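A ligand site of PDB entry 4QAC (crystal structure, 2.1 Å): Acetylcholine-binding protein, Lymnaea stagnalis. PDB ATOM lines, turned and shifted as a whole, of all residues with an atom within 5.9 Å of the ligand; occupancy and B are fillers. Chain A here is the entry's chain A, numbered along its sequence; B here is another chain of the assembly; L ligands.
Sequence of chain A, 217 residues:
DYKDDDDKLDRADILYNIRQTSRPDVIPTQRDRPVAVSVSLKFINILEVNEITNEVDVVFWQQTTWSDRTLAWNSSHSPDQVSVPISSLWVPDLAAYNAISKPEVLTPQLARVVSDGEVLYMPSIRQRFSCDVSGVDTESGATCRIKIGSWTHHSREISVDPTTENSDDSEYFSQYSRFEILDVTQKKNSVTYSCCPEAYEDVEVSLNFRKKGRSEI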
ATOM      1  N   TYR A  97      10.649  -5.604  22.708  1.00  0.00           N
ATOM      2  CA  TYR A  97      10.697  -5.134  21.306  1.00  0.00           C
ATOM      3  C   TYR A  97       9.686  -5.851  20.392  1.00  0.00           C
ATOM      4  O   TYR A  97       9.121  -5.247  19.483  1.00  0.00           O
ATOM      5  CB  TYR A  97      12.119  -5.251  20.720  1.00  0.00           C
ATOM      6  CG  TYR A  97      13.237  -4.609  21.530  1.00  0.00           C
ATOM      7  CD1 TYR A  97      13.002  -3.524  22.382  1.00  0.00           C
ATOM      8  CD2 TYR A  97      14.536  -5.083  21.421  1.00  0.00           C
ATOM      9  CE1 TYR A  97      14.041  -2.950  23.115  1.00  0.00           C
ATOM     10  CE2 TYR A  97      15.578  -4.511  22.136  1.00  0.00           C
ATOM     11  CZ  TYR A  97      15.332  -3.448  22.987  1.00  0.00           C
ATOM     12  OH  TYR A  97      16.378  -2.904  23.687  1.00  0.00           O
ATOM     13  N   GLY A 149      14.501  -4.379  26.754  1.00  0.00           N
ATOM     14  CA  GLY A 149      15.560  -3.433  27.023  1.00  0.00           C
ATOM     15  C   GLY A 149      15.029  -2.061  27.362  1.00  0.00           C
ATOM     16  O   GLY A 149      13.862  -1.773  27.130  1.00  0.00           O
ATOM     17  N   SER A 150      15.876  -1.194  27.922  1.00  0.00           N
ATOM     18  CA  SER A 150      15.493   0.195  28.125  1.00  0.00           C
ATOM     19  C   SER A 150      15.154   0.855  26.782  1.00  0.00           C
ATOM     20  O   SER A 150      15.906   0.725  25.810  1.00  0.00           O
ATOM     21  CB  SER A 150      16.612   0.979  28.810  1.00  0.00           C
ATOM     22  OG  SER A 150      16.267   2.357  28.827  1.00  0.00           O
ATOM     23  N   TRP A 151      14.020   1.549  26.713  1.00  0.00           N
ATOM     24  CA  TRP A 151      13.643   2.179  25.458  1.00  0.00           C
ATOM     25  C   TRP A 151      14.485   3.409  25.148  1.00  0.00           C
ATOM     26  O   TRP A 151      14.966   3.559  24.024  1.00  0.00           O
ATOM     27  CB  TRP A 151      12.144   2.530  25.415  1.00  0.00           C
ATOM     28  CG  TRP A 151      11.615   2.838  23.997  1.00  0.00           C
ATOM     29  CD1 TRP A 151      11.031   4.007  23.575  1.00  0.00           C
ATOM     30  CD2 TRP A 151      11.607   1.955  22.861  1.00  0.00           C
ATOM     31  NE1 TRP A 151      10.664   3.903  22.242  1.00  0.00           N
ATOM     32  CE2 TRP A 151      11.004   2.656  21.786  1.00  0.00           C
ATOM     33  CE3 TRP A 151      12.050   0.652  22.642  1.00  0.00           C
ATOM     34  CZ2 TRP A 151      10.843   2.091  20.513  1.00  0.00           C
ATOM     35  CZ3 TRP A 151      11.876   0.087  21.390  1.00  0.00           C
ATOM     36  CH2 TRP A 151      11.284   0.804  20.340  1.00  0.00           C
ATOM     37  N   THR A 152      14.657   4.286  26.136  1.00  0.00           N
ATOM     38  CA  THR A 152      15.293   5.578  25.828  1.00  0.00           C
ATOM     39  C   THR A 152      16.674   5.752  26.433  1.00  0.00           C
ATOM     40  O   THR A 152      17.375   6.720  26.132  1.00  0.00           O
ATOM     41  CB  THR A 152      14.397   6.794  26.212  1.00  0.00           C
ATOM     42  OG1 THR A 152      14.237   6.870  27.639  1.00  0.00           O
ATOM     43  CG2 THR A 152      13.027   6.700  25.504  1.00  0.00           C
ATOM     44  N   HIS A 153      17.062   4.832  27.298  1.00  0.00           N
ATOM     45  CA  HIS A 153      18.394   4.912  27.893  1.00  0.00           C
ATOM     46  C   HIS A 153      19.317   3.842  27.318  1.00  0.00           C
ATOM     47  O   HIS A 153      19.079   2.644  27.461  1.00  0.00           O
ATOM     48  CB  HIS A 153      18.344   4.832  29.427  1.00  0.00           C
ATOM     49  CG  HIS A 153      17.519   5.905  30.052  1.00  0.00           C
ATOM     50  ND1 HIS A 153      16.193   5.713  30.397  1.00  0.00           N
ATOM     51  CD2 HIS A 153      17.800   7.186  30.379  1.00  0.00           C
ATOM     52  CE1 HIS A 153      15.705   6.827  30.917  1.00  0.00           C
ATOM     53  NE2 HIS A 153      16.667   7.735  30.915  1.00  0.00           N
ATOM     54  N   TYR A 193      21.815   0.342  16.705  1.00  0.00           N
ATOM     55  CA  TYR A 193      20.895   0.399  15.574  1.00  0.00           C
ATOM     56  C   TYR A 193      21.303   1.543  14.649  1.00  0.00           C
ATOM     57  O   TYR A 193      21.953   2.493  15.081  1.00  0.00           O
ATOM     58  CB  TYR A 193      19.459   0.547  16.080  1.00  0.00           C
ATOM     59  CG  TYR A 193      19.082  -0.529  17.073  1.00  0.00           C
ATOM     60  CD1 TYR A 193      18.728  -1.801  16.653  1.00  0.00           C
ATOM     61  CD2 TYR A 193      19.115  -0.285  18.437  1.00  0.00           C
ATOM     62  CE1 TYR A 193      18.404  -2.803  17.565  1.00  0.00           C
ATOM     63  CE2 TYR A 193      18.787  -1.272  19.365  1.00  0.00           C
ATOM     64  CZ  TYR A 193      18.433  -2.525  18.920  1.00  0.00           C
ATOM     65  OH  TYR A 193      18.111  -3.505  19.837  1.00  0.00           O
ATOM     66  N   CYS A 195      19.679   3.844  13.611  1.00  0.00           N
ATOM     67  CA  CYS A 195      19.053   5.080  14.061  1.00  0.00           C
ATOM     68  C   CYS A 195      20.001   5.935  14.903  1.00  0.00           C
ATOM     69  O   CYS A 195      19.981   7.155  14.818  1.00  0.00           O
ATOM     70  CB  CYS A 195      17.800   4.766  14.900  1.00  0.00           C
ATOM     71  SG  CYS A 195      18.181   4.297  16.632  1.00  0.00           S
ATOM     72  N   CYS A 196      20.825   5.264  15.709  1.00  0.00           N
ATOM     73  CA  CYS A 196      21.530   5.939  16.799  1.00  0.00           C
ATOM     74  C   CYS A 196      22.958   5.437  16.959  1.00  0.00           C
ATOM     75  O   CYS A 196      23.238   4.264  16.688  1.00  0.00           O
ATOM     76  CB  CYS A 196      20.779   5.720  18.131  1.00  0.00           C
ATOM     77  SG  CYS A 196      18.965   5.630  17.981  1.00  0.00           S
ATOM     78  N   TYR A 200      22.150  -0.121  22.918  1.00  0.00           N
ATOM     79  CA  TYR A 200      21.048  -0.364  23.849  1.00  0.00           C
ATOM     80  C   TYR A 200      21.108  -1.798  24.308  1.00  0.00           C
ATOM     81  O   TYR A 200      21.032  -2.714  23.490  1.00  0.00           O
ATOM     82  CB  TYR A 200      19.697  -0.102  23.174  1.00  0.00           C
ATOM     83  CG  TYR A 200      19.484   1.337  22.843  1.00  0.00           C
ATOM     84  CD1 TYR A 200      19.930   1.865  21.650  1.00  0.00           C
ATOM     85  CD2 TYR A 200      18.880   2.187  23.755  1.00  0.00           C
ATOM     86  CE1 TYR A 200      19.748   3.206  21.343  1.00  0.00           C
ATOM     87  CE2 TYR A 200      18.698   3.537  23.470  1.00  0.00           C
ATOM     88  CZ  TYR A 200      19.138   4.036  22.266  1.00  0.00           C
ATOM     89  OH  TYR A 200      18.950   5.371  21.969  1.00  0.00           O
ATOM     90  N   GLU A 201      21.229  -1.996  25.612  1.00  0.00           N
ATOM     91  CA  GLU A 201      21.275  -3.341  26.134  1.00  0.00           C
ATOM     92  C   GLU A 201      19.873  -3.956  26.143  1.00  0.00           C
ATOM     93  O   GLU A 201      18.866  -3.249  26.165  1.00  0.00           O
ATOM     94  CB  GLU A 201      21.956  -3.352  27.514  1.00  0.00           C
ATOM     95  CG  GLU A 201      23.409  -2.846  27.450  1.00  0.00           C
ATOM     96  CD  GLU A 201      24.229  -3.117  28.707  1.00  0.00           C
ATOM     97  OE1 GLU A 201      23.723  -3.795  29.618  1.00  0.00           O
ATOM     98  OE2 GLU A 201      25.389  -2.649  28.774  1.00  0.00           O
ATOM     99  N   ILE B  44       7.657  -2.577  11.743  1.00  0.00           N
ATOM    100  CA  ILE B  44       8.100  -3.613  12.661  1.00  0.00           C
ATOM    101  C   ILE B  44       7.385  -4.915  12.292  1.00  0.00           C
ATOM    102  O   ILE B  44       7.953  -6.002  12.377  1.00  0.00           O
ATOM    103  CB  ILE B  44       7.721  -3.282  14.153  1.00  0.00           C
ATOM    104  CG1 ILE B  44       8.330  -1.956  14.605  1.00  0.00           C
ATOM    105  CG2 ILE B  44       8.145  -4.403  15.084  1.00  0.00           C
ATOM    106  CD1 ILE B  44       9.769  -1.814  14.221  1.00  0.00           C
ATOM    107  N   TRP B  61       7.564   1.764  13.859  1.00  0.00           N
ATOM    108  CA  TRP B  61       8.353   2.692  14.634  1.00  0.00           C
ATOM    109  C   TRP B  61       8.194   4.095  14.027  1.00  0.00           C
ATOM    110  O   TRP B  61       8.688   4.352  12.929  1.00  0.00           O
ATOM    111  CB  TRP B  61       9.815   2.280  14.620  1.00  0.00           C
ATOM    112  CG  TRP B  61      10.605   2.981  15.655  1.00  0.00           C
ATOM    113  CD1 TRP B  61      10.116   3.699  16.710  1.00  0.00           C
ATOM    114  CD2 TRP B  61      12.031   3.043  15.768  1.00  0.00           C
ATOM    115  NE1 TRP B  61      11.143   4.189  17.468  1.00  0.00           N
ATOM    116  CE2 TRP B  61      12.342   3.801  16.902  1.00  0.00           C
ATOM    117  CE3 TRP B  61      13.084   2.516  14.997  1.00  0.00           C
ATOM    118  CZ2 TRP B  61      13.659   4.070  17.307  1.00  0.00           C
ATOM    119  CZ3 TRP B  61      14.397   2.777  15.395  1.00  0.00           C
ATOM    120  CH2 TRP B  61      14.671   3.536  16.545  1.00  0.00           C
ATOM    121  N   LEU B 110       8.349   8.481  26.657  1.00  0.00           N
ATOM    122  CA  LEU B 110       9.458   9.352  26.993  1.00  0.00           C
ATOM    123  C   LEU B 110      10.130   9.864  25.718  1.00  0.00           C
ATOM    124  O   LEU B 110      10.341   9.100  24.780  1.00  0.00           O
ATOM    125  CB  LEU B 110      10.501   8.570  27.803  1.00  0.00           C
ATOM    126  CG  LEU B 110      10.091   7.995  29.153  1.00  0.00           C
ATOM    127  CD1 LEU B 110      11.292   7.300  29.849  1.00  0.00           C
ATOM    128  CD2 LEU B 110       9.544   9.113  30.039  1.00  0.00           C
ATOM    129  N   ALA B 111      10.466  11.155  25.696  1.00  0.00           N
ATOM    130  CA  ALA B 111      11.241  11.725  24.581  1.00  0.00           C
ATOM    131  C   ALA B 111      12.690  11.904  25.017  1.00  0.00           C
ATOM    132  O   ALA B 111      12.993  11.837  26.210  1.00  0.00           O
ATOM    133  CB  ALA B 111      10.646  13.063  24.153  1.00  0.00           C
ATOM    134  N   ARG B 112      13.579  12.109  24.050  1.00  0.00           N
ATOM    135  CA  ARG B 112      14.932  12.577  24.357  1.00  0.00           C
ATOM    136  C   ARG B 112      15.031  14.061  24.012  1.00  0.00           C
ATOM    137  O   ARG B 112      14.556  14.503  22.964  1.00  0.00           O
ATOM    138  CB  ARG B 112      16.006  11.782  23.593  1.00  0.00           C
ATOM    139  CG  ARG B 112      16.181  10.350  24.063  1.00  0.00           C
ATOM    140  CD  ARG B 112      16.786  10.296  25.447  1.00  0.00           C
ATOM    141  NE  ARG B 112      18.244  10.294  25.411  1.00  0.00           N
ATOM    142  CZ  ARG B 112      18.999   9.910  26.424  1.00  0.00           C
ATOM    143  NH1 ARG B 112      18.413   9.497  27.541  1.00  0.00           N
ATOM    144  NH2 ARG B 112      20.335   9.918  26.333  1.00  0.00           N
ATOM    145  N   LEU B 120      13.575  14.405  20.277  1.00  0.00           N
ATOM    146  CA  LEU B 120      13.280  13.200  19.517  1.00  0.00           C
ATOM    147  C   LEU B 120      12.232  12.365  20.242  1.00  0.00           C
ATOM    148  O   LEU B 120      12.407  11.997  21.401  1.00  0.00           O
ATOM    149  CB  LEU B 120      14.547  12.372  19.296  1.00  0.00           C
ATOM    150  CG  LEU B 120      15.836  12.907  19.929  1.00  0.00           C
ATOM    151  CD1 LEU B 120      16.975  11.929  19.718  1.00  0.00           C
ATOM    152  CD2 LEU B 120      16.180  14.274  19.350  1.00  0.00           C
ATOM    153  N   TYR B 121      11.147  12.076  19.544  1.00  0.00           N
ATOM    154  CA  TYR B 121      10.133  11.166  20.050  1.00  0.00           C
ATOM    155  C   TYR B 121      10.040  10.028  19.051  1.00  0.00           C
ATOM    156  O   TYR B 121       9.877  10.252  17.849  1.00  0.00           O
ATOM    157  CB  TYR B 121       8.786  11.867  20.167  1.00  0.00           C
ATOM    158  CG  TYR B 121       7.743  11.061  20.903  1.00  0.00           C
ATOM    159  CD1 TYR B 121       8.085  10.266  21.983  1.00  0.00           C
ATOM    160  CD2 TYR B 121       6.408  11.106  20.520  1.00  0.00           C
ATOM    161  CE1 TYR B 121       7.127   9.528  22.662  1.00  0.00           C
ATOM    162  CE2 TYR B 121       5.445  10.367  21.187  1.00  0.00           C
ATOM    163  CZ  TYR B 121       5.813   9.586  22.253  1.00  0.00           C
ATOM    164  OH  TYR B 121       4.853   8.855  22.926  1.00  0.00           O
ATOM    165  N   MET B 122      10.161   8.802  19.541  1.00  0.00           N
ATOM    166  CA  MET B 122      10.113   7.655  18.646  1.00  0.00           C
ATOM    167  C   MET B 122       9.417   6.428  19.263  1.00  0.00           C
ATOM    168  O   MET B 122      10.075   5.456  19.626  1.00  0.00           O
ATOM    169  CB  MET B 122      11.539   7.311  18.172  1.00  0.00           C
ATOM    170  CG  MET B 122      12.342   8.516  17.649  1.00  0.00           C
ATOM    171  SD  MET B 122      13.831   7.982  16.803  1.00  0.00           S
ATOM    172  CE  MET B 122      14.752   9.493  16.690  1.00  0.00           C
ATOM    173  N   SER B 124       6.933   3.033  19.383  1.00  0.00           N
ATOM    174  CA  SER B 124       6.479   1.915  18.556  1.00  0.00           C
ATOM    175  C   SER B 124       4.967   1.879  18.696  1.00  0.00           C
ATOM    176  O   SER B 124       4.417   1.941  19.807  1.00  0.00           O
ATOM    177  CB  SER B 124       7.128   0.617  19.058  1.00  0.00           C
ATOM    178  OG  SER B 124       6.589  -0.495  18.362  1.00  0.00           O
ATOM    179  N   TYR B 172      14.111  -3.283  10.870  1.00  0.00           N
ATOM    180  CA  TYR B 172      13.440  -3.561  12.139  1.00  0.00           C
ATOM    181  C   TYR B 172      12.239  -4.482  11.970  1.00  0.00           C
ATOM    182  O   TYR B 172      11.532  -4.791  12.932  1.00  0.00           O
ATOM    183  CB  TYR B 172      13.030  -2.248  12.807  1.00  0.00           C
ATOM    184  CG  TYR B 172      14.139  -1.234  12.888  1.00  0.00           C
ATOM    185  CD1 TYR B 172      15.242  -1.456  13.693  1.00  0.00           C
ATOM    186  CD2 TYR B 172      14.092  -0.071  12.145  1.00  0.00           C
ATOM    187  CE1 TYR B 172      16.270  -0.529  13.768  1.00  0.00           C
ATOM    188  CE2 TYR B 172      15.105   0.856  12.211  1.00  0.00           C
ATOM    189  CZ  TYR B 172      16.190   0.620  13.025  1.00  0.00           C
ATOM    190  OH  TYR B 172      17.203   1.561  13.090  1.00  0.00           O
HETATM  191  C1  LIG L   1      14.371  -2.057  19.129  1.00  0.00           C
HETATM  192  C2  LIG L   1      13.974  -2.767  17.844  1.00  0.00           C
HETATM  193  C3  LIG L   1      13.215  -1.851  16.856  1.00  0.00           C
HETATM  194  C4  LIG L   1      11.710  -1.938  17.088  1.00  0.00           C
HETATM  195  C5  LIG L   1      13.701  -0.407  17.022  1.00  0.00           C
HETATM  196  C6  LIG L   1      15.148  -0.354  17.483  1.00  0.00           C
HETATM  197  N1  LIG L   1      15.264  -0.866  18.861  1.00  0.00           N
HETATM  198  C7  LIG L   1      15.353   0.130  19.855  1.00  0.00           C
HETATM  199  C8  LIG L   1      15.130   1.536  19.700  1.00  0.00           C
HETATM  200  N2  LIG L   1      15.661  -0.417  21.074  1.00  0.00           N
HETATM  201  C9  LIG L   1      15.761   0.476  22.122  1.00  0.00           C
HETATM  202  N3  LIG L   1      16.083  -0.063  23.373  1.00  0.00           N
HETATM  203  N4  LIG L   1      15.573   1.810  22.073  1.00  0.00           N
HETATM  204  C10 LIG L   1      15.259   2.337  20.866  1.00  0.00           C
HETATM  205  C11 LIG L   1      15.069   3.824  20.909  1.00  0.00           C
HETATM  206  C12 LIG L   1      16.177   4.690  20.744  1.00  0.00           C
HETATM  207  C13 LIG L   1      16.038   6.081  20.832  1.00  0.00           C
HETATM  208  C14 LIG L   1      14.782   6.635  21.088  1.00  0.00           C
HETATM  209  C15 LIG L   1      14.596   8.149  21.213  1.00  0.00           C
HETATM  210  F1  LIG L   1      13.516   8.656  20.575  1.00  0.00           F
HETATM  211  F2  LIG L   1      15.657   8.896  20.820  1.00  0.00           F
HETATM  212  F3  LIG L   1      14.377   8.499  22.495  1.00  0.00           F
HETATM  213  C16 LIG L   1      13.688   5.807  21.283  1.00  0.00           C
HETATM  214  C17 LIG L   1      13.827   4.415  21.195  1.00  0.00           C
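The backbone NH of His 153 sits at hydrogen-bond distance from the side-chain hydroxyl of Ser 150, at 3.0 Å. The backbone carbonyl oxygen (O) of Met 122 of chain B is in hydrogen-bond range of the indole nitrogen (NE1) of Trp 151, 3.1 Å away. O of Arg 112 of chain B lies within hydrogen-bond range of N of Leu 120 of chain B (2.9 Å). O of Thr 152 lies within hydrogen-bond range of NH1 of Arg 112 of chain B, at 3.3 Å. The indole nitrogen (NE1) of Trp 61 of chain B is in hydrogen-bond range of the backbone carbonyl oxygen (O) of Met 122 of chain B (2.7 Å). OH of Tyr 172 of chain B sits at hydrogen-bond distance from N of Cys 195. SG of Cys 196 is disulfide-bonded to SG of Cys 195, 2.1 Å away.
Merely in contact with the ligand: Thr 152 (3.8 Å), Tyr 193 (3.6 Å), Tyr 200 (3.1 Å), Ile 44 of chain B (3.5 Å), Trp 61 of chain B (3.6 Å), Arg 112 of chain B (3.0 Å), Leu 120 of chain B (3.5 Å), Met 122 of chain B (3.2 Å) and Tyr 172 of chain B (3.8 Å). Hydrophobic or aromatic side chains within 4 Å of the ligand: Tyr 97, Trp 151, Tyr 193, Tyr 200, Ile 44 of chain B, Trp 61 of chain B, Leu 120 of chain B, Met 122 of chain B and Tyr 172 of chain B. Within 4 Å of the ligand: Tyr 97, Ser 150, Trp 151, Thr 152, Tyr 193, Tyr 200, Ile 44 of chain B, Trp 61 of chain B, Arg 112 of chain B, Leu 120 of chain B, Met 122 of chain B and Tyr 172 of chain B.
O of Ser 150 lies within hydrogen-bond range of N3 of the ligand (2.6 Å). O of Trp 151 lies close to N4 of the ligand. N3 of the ligand sits at hydrogen-bond distance from OH of Tyr 97 (2.9 Å).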
